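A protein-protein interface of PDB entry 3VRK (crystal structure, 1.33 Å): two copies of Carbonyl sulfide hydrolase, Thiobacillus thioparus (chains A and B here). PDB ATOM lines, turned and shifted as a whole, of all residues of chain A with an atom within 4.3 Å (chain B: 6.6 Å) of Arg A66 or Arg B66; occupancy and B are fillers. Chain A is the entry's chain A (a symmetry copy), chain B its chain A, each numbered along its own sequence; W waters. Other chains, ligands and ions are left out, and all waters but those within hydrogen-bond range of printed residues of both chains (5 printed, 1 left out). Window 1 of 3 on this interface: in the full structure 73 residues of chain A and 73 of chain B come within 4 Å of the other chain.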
ATOM      1  N   ALA A  43      -5.931 -25.342 -13.655  1.00  0.00           N
ATOM      2  CA  ALA A  43      -6.554 -24.560 -14.739  1.00  0.00           C
ATOM      3  C   ALA A  43      -5.961 -23.174 -14.783  1.00  0.00           C
ATOM      4  O   ALA A  43      -5.274 -22.721 -13.848  1.00  0.00           O
ATOM      5  CB  ALA A  43      -8.056 -24.447 -14.529  1.00  0.00           C
ATOM      6  N   CYS A  44      -6.232 -22.425 -15.858  1.00  0.00           N
ATOM      7  CA  CYS A  44      -5.840 -21.021 -15.928  1.00  0.00           C
ATOM      8  C   CYS A  44      -6.666 -20.176 -14.961  1.00  0.00           C
ATOM      9  O   CYS A  44      -7.824 -20.500 -14.679  1.00  0.00           O
ATOM     10  CB  CYS A  44      -6.013 -20.498 -17.361  1.00  0.00           C
ATOM     11  SG  CYS A  44      -5.288 -18.812 -17.518  1.00  0.00           S
ATOM     12  N   MET A  45      -6.081 -19.095 -14.450  1.00  0.00           N
ATOM     13  CA  MET A  45      -6.757 -18.088 -13.617  1.00  0.00           C
ATOM     14  C   MET A  45      -7.746 -17.238 -14.399  1.00  0.00           C
ATOM     15  O   MET A  45      -8.471 -16.455 -13.746  1.00  0.00           O
ATOM     16  CB  MET A  45      -5.714 -17.157 -12.974  1.00  0.00           C
ATOM     17  CG  MET A  45      -5.047 -16.218 -13.995  1.00  0.00           C
ATOM     18  SD  MET A  45      -3.829 -15.152 -13.187  1.00  0.00           S
ATOM     19  CE  MET A  45      -3.512 -13.949 -14.481  1.00  0.00           C
ATOM     20  N   ASP A  46      -7.799 -17.364 -15.712  1.00  0.00           N
ATOM     21  CA  ASP A  46      -8.639 -16.555 -16.556  1.00  0.00           C
ATOM     22  C   ASP A  46     -10.064 -16.445 -16.009  1.00  0.00           C
ATOM     23  O   ASP A  46     -10.678 -17.454 -15.631  1.00  0.00           O
ATOM     24  CB  ASP A  46      -8.673 -17.207 -17.958  1.00  0.00           C
ATOM     25  CG  ASP A  46      -9.347 -16.377 -19.022  1.00  0.00           C
ATOM     26  OD1 ASP A  46     -10.589 -16.221 -18.951  1.00  0.00           O
ATOM     27  OD2 ASP A  46      -8.654 -15.901 -19.953  1.00  0.00           O
ATOM     28  N   LEU A  49     -13.127 -18.712 -16.801  1.00  0.00           N
ATOM     29  CA  LEU A  49     -13.230 -20.094 -16.348  1.00  0.00           C
ATOM     30  C   LEU A  49     -13.762 -20.075 -14.914  1.00  0.00           C
ATOM     31  O   LEU A  49     -13.147 -19.473 -14.022  1.00  0.00           O
ATOM     32  CB  LEU A  49     -11.895 -20.813 -16.323  1.00  0.00           C
ATOM     33  CG  LEU A  49     -11.438 -21.423 -17.649  1.00  0.00           C
ATOM     34  CD1 LEU A  49     -11.211 -20.311 -18.637  1.00  0.00           C
ATOM     35  CD2 LEU A  49     -10.197 -22.251 -17.405  1.00  0.00           C
ATOM     36  N   VAL A  51     -14.124 -23.190 -12.795  1.00  0.00           N
ATOM     37  CA  VAL A  51     -13.714 -24.582 -12.993  1.00  0.00           C
ATOM     38  C   VAL A  51     -14.787 -25.543 -12.490  1.00  0.00           C
ATOM     39  O   VAL A  51     -15.163 -26.530 -13.157  1.00  0.00           O
ATOM     40  CB  VAL A  51     -12.355 -24.862 -12.330  1.00  0.00           C
ATOM     41  CG1 VAL A  51     -11.965 -26.314 -12.434  1.00  0.00           C
ATOM     42  CG2 VAL A  51     -11.276 -23.977 -12.997  1.00  0.00           C
ATOM     43  N   GLU A  52     -15.332 -25.244 -11.301  1.00  0.00           N
ATOM     44  CA  GLU A  52     -16.377 -26.083 -10.722  1.00  0.00           C
ATOM     45  C   GLU A  52     -17.566 -26.071 -11.678  1.00  0.00           C
ATOM     46  O   GLU A  52     -18.158 -27.128 -11.954  1.00  0.00           O
ATOM     47  CB  GLU A  52     -16.760 -25.640  -9.315  1.00  0.00           C
ATOM     48  CG  GLU A  52     -15.561 -25.717  -8.331  1.00  0.00           C
ATOM     49  CD  GLU A  52     -14.833 -24.397  -8.149  1.00  0.00           C
ATOM     50  OE1 GLU A  52     -14.887 -23.528  -9.057  1.00  0.00           O
ATOM     51  OE2 GLU A  52     -14.169 -24.228  -7.111  1.00  0.00           O
ATOM     52  N   ILE A  64      -8.771 -27.345  -6.576  1.00  0.00           N
ATOM     53  CA  ILE A  64      -8.801 -26.416  -7.706  1.00  0.00           C
ATOM     54  C   ILE A  64      -7.552 -25.531  -7.646  1.00  0.00           C
ATOM     55  O   ILE A  64      -7.470 -24.702  -6.744  1.00  0.00           O
ATOM     56  CB  ILE A  64     -10.079 -25.558  -7.641  1.00  0.00           C
ATOM     57  CG1 ILE A  64     -11.375 -26.358  -7.444  1.00  0.00           C
ATOM     58  CG2 ILE A  64     -10.179 -24.702  -8.912  1.00  0.00           C
ATOM     59  CD1 ILE A  64     -11.704 -27.330  -8.562  1.00  0.00           C
ATOM     60  N   ILE A  65      -6.618 -25.817  -8.542  1.00  0.00           N
ATOM     61  CA  ILE A  65      -5.316 -25.139  -8.581  1.00  0.00           C
ATOM     62  C   ILE A  65      -5.334 -24.272  -9.811  1.00  0.00           C
ATOM     63  O   ILE A  65      -5.631 -24.761 -10.907  1.00  0.00           O
ATOM     64  CB  ILE A  65      -4.187 -26.189  -8.640  1.00  0.00           C
ATOM     65  CG1 ILE A  65      -4.211 -27.103  -7.423  1.00  0.00           C
ATOM     66  CG2 ILE A  65      -2.840 -25.485  -8.834  1.00  0.00           C
ATOM     67  CD1 ILE A  65      -3.561 -28.473  -7.706  1.00  0.00           C
ATOM     68  N   ARG A  66      -5.089 -22.967  -9.654  1.00  0.00           N
ATOM     69  CA  ARG A  66      -5.209 -22.063 -10.824  1.00  0.00           C
ATOM     70  C   ARG A  66      -4.079 -21.035 -10.851  1.00  0.00           C
ATOM     71  O   ARG A  66      -3.786 -20.421  -9.823  1.00  0.00           O
ATOM     72  CB  ARG A  66      -6.548 -21.333 -10.838  1.00  0.00           C
ATOM     73  CG  ARG A  66      -7.754 -22.296 -10.836  1.00  0.00           C
ATOM     74  CD  ARG A  66      -9.150 -21.655 -10.906  1.00  0.00           C
ATOM     75  NE  ARG A  66      -9.253 -20.890 -12.168  1.00  0.00           N
ATOM     76  CZ  ARG A  66     -10.317 -20.164 -12.492  1.00  0.00           C
ATOM     77  NH1 ARG A  66     -11.395 -20.162 -11.715  1.00  0.00           N
ATOM     78  NH2 ARG A  66     -10.319 -19.452 -13.616  1.00  0.00           N
ATOM     79  N   ASN A  67      -3.507 -20.854 -12.046  1.00  0.00           N
ATOM     80  CA  ASN A  67      -2.413 -19.873 -12.182  1.00  0.00           C
ATOM     81  C   ASN A  67      -2.453 -19.296 -13.589  1.00  0.00           C
ATOM     82  O   ASN A  67      -3.284 -19.738 -14.417  1.00  0.00           O
ATOM     83  CB  ASN A  67      -1.057 -20.511 -11.830  1.00  0.00           C
ATOM     84  CG  ASN A  67      -0.648 -21.598 -12.809  1.00  0.00           C
ATOM     85  OD1 ASN A  67      -0.864 -21.467 -14.029  1.00  0.00           O
ATOM     86  ND2 ASN A  67      -0.033 -22.661 -12.313  1.00  0.00           N
ATOM     87  N   VAL B  41      -8.281 -12.662  -7.173  1.00  0.00           N
ATOM     88  CA  VAL B  41      -8.423 -13.282  -5.865  1.00  0.00           C
ATOM     89  C   VAL B  41      -7.360 -14.370  -5.758  1.00  0.00           C
ATOM     90  O   VAL B  41      -7.184 -15.143  -6.704  1.00  0.00           O
ATOM     91  CB  VAL B  41      -9.818 -13.929  -5.683  1.00  0.00           C
ATOM     92  CG1 VAL B  41      -9.985 -14.492  -4.275  1.00  0.00           C
ATOM     93  CG2 VAL B  41     -10.943 -12.955  -6.003  1.00  0.00           C
ATOM     94  N   VAL B  42      -6.655 -14.448  -4.633  1.00  0.00           N
ATOM     95  CA  VAL B  42      -5.704 -15.545  -4.390  1.00  0.00           C
ATOM     96  C   VAL B  42      -6.269 -16.349  -3.225  1.00  0.00           C
ATOM     97  O   VAL B  42      -6.454 -15.782  -2.130  1.00  0.00           O
ATOM     98  CB  VAL B  42      -4.298 -15.071  -4.026  1.00  0.00           C
ATOM     99  CG1 VAL B  42      -3.395 -16.307  -3.819  1.00  0.00           C
ATOM    100  CG2 VAL B  42      -3.744 -14.150  -5.107  1.00  0.00           C
ATOM    101  N   ALA B  43      -6.546 -17.638  -3.457  1.00  0.00           N
ATOM    102  CA  ALA B  43      -7.208 -18.456  -2.424  1.00  0.00           C
ATOM    103  C   ALA B  43      -6.544 -19.809  -2.331  1.00  0.00           C
ATOM    104  O   ALA B  43      -5.762 -20.220  -3.208  1.00  0.00           O
ATOM    105  CB  ALA B  43      -8.680 -18.652  -2.751  1.00  0.00           C
ATOM    106  N   CYS B  44      -6.857 -20.573  -1.280  1.00  0.00           N
ATOM    107  CA  CYS B  44      -6.394 -21.954  -1.175  1.00  0.00           C
ATOM    108  C   CYS B  44      -7.093 -22.841  -2.202  1.00  0.00           C
ATOM    109  O   CYS B  44      -8.243 -22.580  -2.575  1.00  0.00           O
ATOM    110  CB  CYS B  44      -6.650 -22.489   0.241  1.00  0.00           C
ATOM    111  SG  CYS B  44      -5.847 -24.132   0.457  1.00  0.00           S
ATOM    112  N   MET B  45      -6.411 -23.886  -2.664  1.00  0.00           N
ATOM    113  CA  MET B  45      -6.963 -24.928  -3.545  1.00  0.00           C
ATOM    114  C   MET B  45      -7.963 -25.832  -2.842  1.00  0.00           C
ATOM    115  O   MET B  45      -8.589 -26.652  -3.547  1.00  0.00           O
ATOM    116  CB  MET B  45      -5.824 -25.798  -4.102  1.00  0.00           C
ATOM    117  CG  MET B  45      -5.187 -26.699  -3.030  1.00  0.00           C
ATOM    118  SD  MET B  45      -3.852 -27.696  -3.738  1.00  0.00           S
ATOM    119  CE  MET B  45      -3.572 -28.882  -2.419  1.00  0.00           C
ATOM    120  N   ASP B  46      -8.124 -25.712  -1.538  1.00  0.00           N
ATOM    121  CA  ASP B  46      -8.982 -26.569  -0.759  1.00  0.00           C
ATOM    122  C   ASP B  46     -10.351 -26.756  -1.416  1.00  0.00           C
ATOM    123  O   ASP B  46     -10.989 -25.781  -1.842  1.00  0.00           O
ATOM    124  CB  ASP B  46      -9.163 -25.922   0.635  1.00  0.00           C
ATOM    125  CG  ASP B  46      -9.870 -26.792   1.644  1.00  0.00           C
ATOM    126  OD1 ASP B  46     -11.093 -27.016   1.476  1.00  0.00           O
ATOM    127  OD2 ASP B  46      -9.227 -27.230   2.627  1.00  0.00           O
ATOM    128  N   ALA B  47     -10.769 -28.011  -1.524  1.00  0.00           N
ATOM    129  CA  ALA B  47     -11.992 -28.333  -2.281  1.00  0.00           C
ATOM    130  C   ALA B  47     -13.222 -27.652  -1.728  1.00  0.00           C
ATOM    131  O   ALA B  47     -14.202 -27.445  -2.447  1.00  0.00           O
ATOM    132  CB  ALA B  47     -12.198 -29.842  -2.264  1.00  0.00           C
ATOM    133  N   ARG B  48     -13.201 -27.302  -0.450  1.00  0.00           N
ATOM    134  CA  ARG B  48     -14.384 -26.712   0.197  1.00  0.00           C
ATOM    135  C   ARG B  48     -14.563 -25.254  -0.173  1.00  0.00           C
ATOM    136  O   ARG B  48     -15.588 -24.652   0.191  1.00  0.00           O
ATOM    137  CB  ARG B  48     -14.267 -26.892   1.719  1.00  0.00           C
ATOM    138  CG  ARG B  48     -14.170 -28.365   2.131  1.00  0.00           C
ATOM    139  CD  ARG B  48     -13.868 -28.523   3.616  1.00  0.00           C
ATOM    140  NE  ARG B  48     -12.453 -28.164   3.847  1.00  0.00           N
ATOM    141  CZ  ARG B  48     -11.822 -28.371   4.979  1.00  0.00           C
ATOM    142  NH1 ARG B  48     -12.431 -28.933   6.022  1.00  0.00           N
ATOM    143  NH2 ARG B  48     -10.535 -28.012   5.059  1.00  0.00           N
ATOM    144  N   LEU B  49     -13.589 -24.665  -0.871  1.00  0.00           N
ATOM    145  CA  LEU B  49     -13.731 -23.289  -1.334  1.00  0.00           C
ATOM    146  C   LEU B  49     -14.147 -23.334  -2.805  1.00  0.00           C
ATOM    147  O   LEU B  49     -13.433 -23.900  -3.645  1.00  0.00           O
ATOM    148  CB  LEU B  49     -12.441 -22.498  -1.257  1.00  0.00           C
ATOM    149  CG  LEU B  49     -12.124 -21.865   0.100  1.00  0.00           C
ATOM    150  CD1 LEU B  49     -11.913 -22.965   1.104  1.00  0.00           C
ATOM    151  CD2 LEU B  49     -10.915 -20.970  -0.049  1.00  0.00           C
ATOM    152  N   ASP B  50     -15.299 -22.732  -3.103  1.00  0.00           N
ATOM    153  CA  ASP B  50     -15.622 -22.326  -4.481  1.00  0.00           C
ATOM    154  C   ASP B  50     -15.574 -20.805  -4.395  1.00  0.00           C
ATOM    155  O   ASP B  50     -16.441 -20.180  -3.775  1.00  0.00           O
ATOM    156  CB  ASP B  50     -16.988 -22.862  -4.950  1.00  0.00           C
ATOM    157  CG  ASP B  50     -17.208 -22.478  -6.416  1.00  0.00           C
ATOM    158  OD1 ASP B  50     -17.081 -21.262  -6.689  1.00  0.00           O
ATOM    159  OD2 ASP B  50     -17.470 -23.348  -7.273  1.00  0.00           O
ATOM    160  N   VAL B  51     -14.515 -20.240  -4.953  1.00  0.00           N
ATOM    161  CA  VAL B  51     -14.199 -18.828  -4.727  1.00  0.00           C
ATOM    162  C   VAL B  51     -15.282 -17.927  -5.314  1.00  0.00           C
ATOM    163  O   VAL B  51     -15.762 -16.963  -4.681  1.00  0.00           O
ATOM    164  CB  VAL B  51     -12.809 -18.471  -5.282  1.00  0.00           C
ATOM    165  CG1 VAL B  51     -12.511 -17.000  -5.150  1.00  0.00           C
ATOM    166  CG2 VAL B  51     -11.739 -19.297  -4.530  1.00  0.00           C
ATOM    167  N   GLU B  52     -15.713 -18.253  -6.542  1.00  0.00           N
ATOM    168  CA  GLU B  52     -16.754 -17.472  -7.203  1.00  0.00           C
ATOM    169  C   GLU B  52     -18.012 -17.551  -6.343  1.00  0.00           C
ATOM    170  O   GLU B  52     -18.681 -16.529  -6.117  1.00  0.00           O
ATOM    171  CB  GLU B  52     -17.001 -17.933  -8.634  1.00  0.00           C
ATOM    172  CG  GLU B  52     -15.734 -17.787  -9.523  1.00  0.00           C
ATOM    173  CD  GLU B  52     -14.923 -19.064  -9.643  1.00  0.00           C
ATOM    174  OE1 GLU B  52     -14.999 -19.937  -8.740  1.00  0.00           O
ATOM    175  OE2 GLU B  52     -14.170 -19.194 -10.626  1.00  0.00           O
ATOM    176  N   ALA B  62     -13.443 -11.898 -12.281  1.00  0.00           N
ATOM    177  CA  ALA B  62     -12.206 -11.822 -11.510  1.00  0.00           C
ATOM    178  C   ALA B  62     -11.228 -12.889 -11.926  1.00  0.00           C
ATOM    179  O   ALA B  62     -11.641 -14.011 -12.247  1.00  0.00           O
ATOM    180  CB  ALA B  62     -12.503 -12.031 -10.011  1.00  0.00           C
ATOM    181  N   HIS B  63      -9.920 -12.554 -11.887  1.00  0.00           N
ATOM    182  CA  HIS B  63      -8.935 -13.650 -11.895  1.00  0.00           C
ATOM    183  C   HIS B  63      -9.050 -14.456 -10.600  1.00  0.00           C
ATOM    184  O   HIS B  63      -9.215 -13.913  -9.504  1.00  0.00           O
ATOM    185  CB  HIS B  63      -7.532 -13.074 -11.997  1.00  0.00           C
ATOM    186  CG  HIS B  63      -7.232 -12.674 -13.408  1.00  0.00           C
ATOM    187  ND1 HIS B  63      -6.542 -11.534 -13.740  1.00  0.00           N
ATOM    188  CD2 HIS B  63      -7.530 -13.313 -14.561  1.00  0.00           C
ATOM    189  CE1 HIS B  63      -6.419 -11.459 -15.067  1.00  0.00           C
ATOM    190  NE2 HIS B  63      -7.018 -12.551 -15.587  1.00  0.00           N
ATOM    191  N   ILE B  64      -8.929 -15.781 -10.742  1.00  0.00           N
ATOM    192  CA  ILE B  64      -8.995 -16.713  -9.616  1.00  0.00           C
ATOM    193  C   ILE B  64      -7.699 -17.526  -9.576  1.00  0.00           C
ATOM    194  O   ILE B  64      -7.499 -18.348 -10.468  1.00  0.00           O
ATOM    195  CB  ILE B  64     -10.215 -17.640  -9.779  1.00  0.00           C
ATOM    196  CG1 ILE B  64     -11.535 -16.912 -10.079  1.00  0.00           C
ATOM    197  CG2 ILE B  64     -10.367 -18.503  -8.518  1.00  0.00           C
ATOM    198  CD1 ILE B  64     -12.002 -15.963  -8.992  1.00  0.00           C
ATOM    199  N   ILE B  65      -6.854 -17.191  -8.609  1.00  0.00           N
ATOM    200  CA  ILE B  65      -5.524 -17.796  -8.469  1.00  0.00           C
ATOM    201  C   ILE B  65      -5.591 -18.666  -7.241  1.00  0.00           C
ATOM    202  O   ILE B  65      -5.999 -18.196  -6.172  1.00  0.00           O
ATOM    203  CB  ILE B  65      -4.464 -16.686  -8.322  1.00  0.00           C
ATOM    204  CG1 ILE B  65      -4.443 -15.772  -9.541  1.00  0.00           C
ATOM    205  CG2 ILE B  65      -3.098 -17.314  -8.023  1.00  0.00           C
ATOM    206  CD1 ILE B  65      -3.894 -14.369  -9.210  1.00  0.00           C
ATOM    207  N   ARG B  66      -5.262 -19.955  -7.376  1.00  0.00           N
ATOM    208  CA  ARG B  66      -5.424 -20.867  -6.216  1.00  0.00           C
ATOM    209  C   ARG B  66      -4.244 -21.830  -6.098  1.00  0.00           C
ATOM    210  O   ARG B  66      -3.838 -22.424  -7.098  1.00  0.00           O
ATOM    211  CB  ARG B  66      -6.717 -21.669  -6.305  1.00  0.00           C
ATOM    212  CG  ARG B  66      -7.971 -20.775  -6.404  1.00  0.00           C
ATOM    213  CD  ARG B  66      -9.331 -21.492  -6.442  1.00  0.00           C
ATOM    214  NE  ARG B  66      -9.489 -22.265  -5.192  1.00  0.00           N
ATOM    215  CZ  ARG B  66     -10.534 -23.050  -4.950  1.00  0.00           C
ATOM    216  NH1 ARG B  66     -11.546 -23.109  -5.809  1.00  0.00           N
ATOM    217  NH2 ARG B  66     -10.585 -23.763  -3.828  1.00  0.00           N
ATOM    218  N   ASN B  67      -3.758 -21.983  -4.862  1.00  0.00           N
ATOM    219  CA  ASN B  67      -2.627 -22.902  -4.638  1.00  0.00           C
ATOM    220  C   ASN B  67      -2.743 -23.483  -3.237  1.00  0.00           C
ATOM    221  O   ASN B  67      -3.661 -23.089  -2.478  1.00  0.00           O
ATOM    222  CB  ASN B  67      -1.282 -22.188  -4.884  1.00  0.00           C
ATOM    223  CG  ASN B  67      -1.014 -21.084  -3.878  1.00  0.00           C
ATOM    224  OD1 ASN B  67      -1.316 -21.228  -2.679  1.00  0.00           O
ATOM    225  ND2 ASN B  67      -0.421 -19.985  -4.328  1.00  0.00           N
ATOM    226  N   ALA B  68      -1.851 -24.344  -2.794  1.00  0.00           N
ATOM    227  CA  ALA B  68      -1.968 -24.920  -1.445  1.00  0.00           C
ATOM    228  C   ALA B  68      -1.658 -23.852  -0.402  1.00  0.00           C
ATOM    229  O   ALA B  68      -0.502 -23.383  -0.323  1.00  0.00           O
ATOM    230  CB  ALA B  68      -1.048 -26.127  -1.348  1.00  0.00           C
ATOM    231  N   GLY B  70      -3.193 -20.841  -0.480  1.00  0.00           N
ATOM    232  CA  GLY B  70      -3.437 -19.477  -0.945  1.00  0.00           C
ATOM    233  C   GLY B  70      -2.230 -18.609  -0.643  1.00  0.00           C
ATOM    234  O   GLY B  70      -2.379 -17.393  -0.395  1.00  0.00           O
ATOM    235  N   ASP B  75       5.056 -17.952  -7.825  1.00  0.00           N
ATOM    236  CA  ASP B  75       4.010 -18.112  -8.832  1.00  0.00           C
ATOM    237  C   ASP B  75       2.857 -17.149  -8.578  1.00  0.00           C
ATOM    238  O   ASP B  75       2.307 -16.601  -9.532  1.00  0.00           O
ATOM    239  CB  ASP B  75       3.505 -19.559  -8.810  1.00  0.00           C
ATOM    240  CG  ASP B  75       2.373 -19.822  -9.797  1.00  0.00           C
ATOM    241  OD1 ASP B  75       2.519 -19.716 -11.007  1.00  0.00           O
ATOM    242  OD2 ASP B  75       1.267 -20.184  -9.371  1.00  0.00           O
ATOM    243  N   CYS B  79       1.474 -14.521 -11.339  1.00  0.00           N
ATOM    244  CA  CYS B  79       0.069 -14.350 -11.722  1.00  0.00           C
ATOM    245  C   CYS B  79      -0.441 -12.924 -11.556  1.00  0.00           C
ATOM    246  O   CYS B  79      -1.153 -12.386 -12.419  1.00  0.00           O
ATOM    247  CB  CYS B  79      -0.824 -15.279 -10.855  1.00  0.00           C
ATOM    248  SG  CYS B  79      -0.586 -17.043 -11.134  1.00  0.00           S
HETATM  249  O   HOH W   1       0.726 -23.395  -9.968  1.00  0.00           O
HETATM  250  O   HOH W   2     -13.345 -21.526  -7.226  1.00  0.00           O
HETATM  251  O   HOH W   3     -14.621 -17.029 -12.581  1.00  0.00           O
HETATM  252  O   HOH W   4     -13.209 -21.846 -10.440  1.00  0.00           O
HETATM  253  O   HOH W   5      -8.866 -13.434 -17.637  1.00  0.00           O
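Of chain B, only Glu B52, Ile B64, Ile B65 and Arg B66 come within 4 Å of Arg A66.
Printed residues of chain A within 4 Å of Arg B66: Glu A52, Ile A64, Ile A65 and Arg A66.
Of the printed residues of chain A, Ile B65 touches Met A45 and Arg A66.
Of the printed residues of chain A, Met B45 touches Ile A64 and Ile A65.
Of the printed residues of chain A, Asp B50 touches Glu A52.
Printed residues of chain B within 4 Å of Glu A52: Leu B49 (3.6 Å), Asp B50 (3.0 Å), Glu B52 (3.6 Å) and Arg B66 (3.1 Å).
Ala B47 touches none of the printed residues of chain A.
His B63 touches Met A45.
Met A45 touches Ile B65.
CE of Met A45 touches O of Cys B79, at 3.5 Å.
Asp A46 touches His B63 (CA to CD2, 3.96 Å).
Leu B49 touches Glu A52.
Glu A52 touches Glu B52 (OE1 to OE1, 3.6 Å).
CG1 of Ile A65 touches SD of Met B45, 3.7 Å away.
CB of Arg A66 touches O of Ile B64, 3.2 Å away.
Asn A67 touches Asp B75 (CB to OD2, 3.4 Å).
CA of Asn A67 touches SG of Cys B79, at 3.5 Å.
The backbone carbonyl oxygen (O) of Met B45 lies within hydrogen-bond range of the backbone NH (N) of Ile A64, at 3.1 Å.
The side-chain carboxylate (OE2) of Glu B52 is in salt-bridge range of the guanidinium group (NH1) of Arg A66, 3.1 Å away.
The backbone NH (N) of Ile B64 is in hydrogen-bond range of the backbone carbonyl oxygen (O) of Met A45, 3.1 Å away.
The guanidinium group of Arg B66 lies within salt-bridge range of the side-chain carboxylate of Glu A52 (3.1 Å).
N of Arg B66 is in hydrogen-bond range of O of Arg A66.
The side-chain carboxylate (OE1) of Glu A52 lies close to the side-chain carboxylate (OD2) of Asp B50, 3.1 Å away.
Met A45 touches Ile B64, and with the chains exchanged Ile A64 touches Met B45.
Met A45 touches Ile B65, and with the chains exchanged Ile A65 touches Met B45.
Glu A52 touches its own counterpart, Glu B52.
Arg B66 touches its own counterpart, Arg A66.
11 positions are printed for both chains.
Of the 20 pairs that touch across the chains among the printed residues, 14 have their exchanged pair printed and touching as well.
The backbone carbonyl oxygen (O) of His B63 lies within hydrogen-bond range of the backbone NH (N) of Val B41 (2.8 Å).
O of Val B41 lies within hydrogen-bond range of N of Ile B65 (2.8 Å).
The guanidinium group of Arg B66 sits at hydrogen-bond distance from the backbone carbonyl oxygen of Cys B44 (2.9 Å).
O of Asp B46 lies within hydrogen-bond range of NH2 of Arg B66 (2.9 Å).
The side-chain carboxylate of Asp B50 sits at hydrogen-bond distance from the backbone NH of Glu B52, at 3.3 Å.
The backbone carbonyl oxygen (O) of Ile A65 sits at hydrogen-bond distance from the backbone NH (N) of Ala A43 (2.8 Å).
Water W1 lies within hydrogen-bond range of the side-chain amide nitrogen (ND2) of Asn A67 (2.6 Å) and the side-chain carboxylate (OD2) of Asp B75 (3.3 Å).
Water W2 lies within hydrogen-bond range of the side-chain carboxylate (OE1) of Glu B52 (2.7 Å), the guanidinium group (NH1) of Arg B66 (2.8 Å), the side-chain carboxylate (OE2) of Glu A52 (2.8 Å) and the backbone NH (N) of Val B51 (2.9 Å).
Water W4 lies within hydrogen-bond range of the side-chain carboxylate (OE1) of Glu A52 (2.7 Å), the guanidinium group (NH1) of Arg A66 (2.8 Å), the side-chain carboxylate (OE2) of Glu B52 (2.8 Å) and the backbone NH (N) of Val A51 (2.9 Å).
Water W5 bridges NE2 of His B63 (2.9 Å) and OD2 of Asp A46 (3.4 Å).
Water W3 bridges OE2 of Glu B52 (3.0 Å) and O of Leu A49 (3.2 Å).
Hydrophobic or aromatic side chains of chain A that line the printed part of chain B: Met A45, Ile A64 and Ile A65.
Among the printed residues, Asp or Glu carboxylates within 4 Å of a Lys or Arg side-chain nitrogen of the other chain: Glu A52 with Arg B66 (3.1 Å) and Arg A66 with Glu B52 (3.1 Å).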
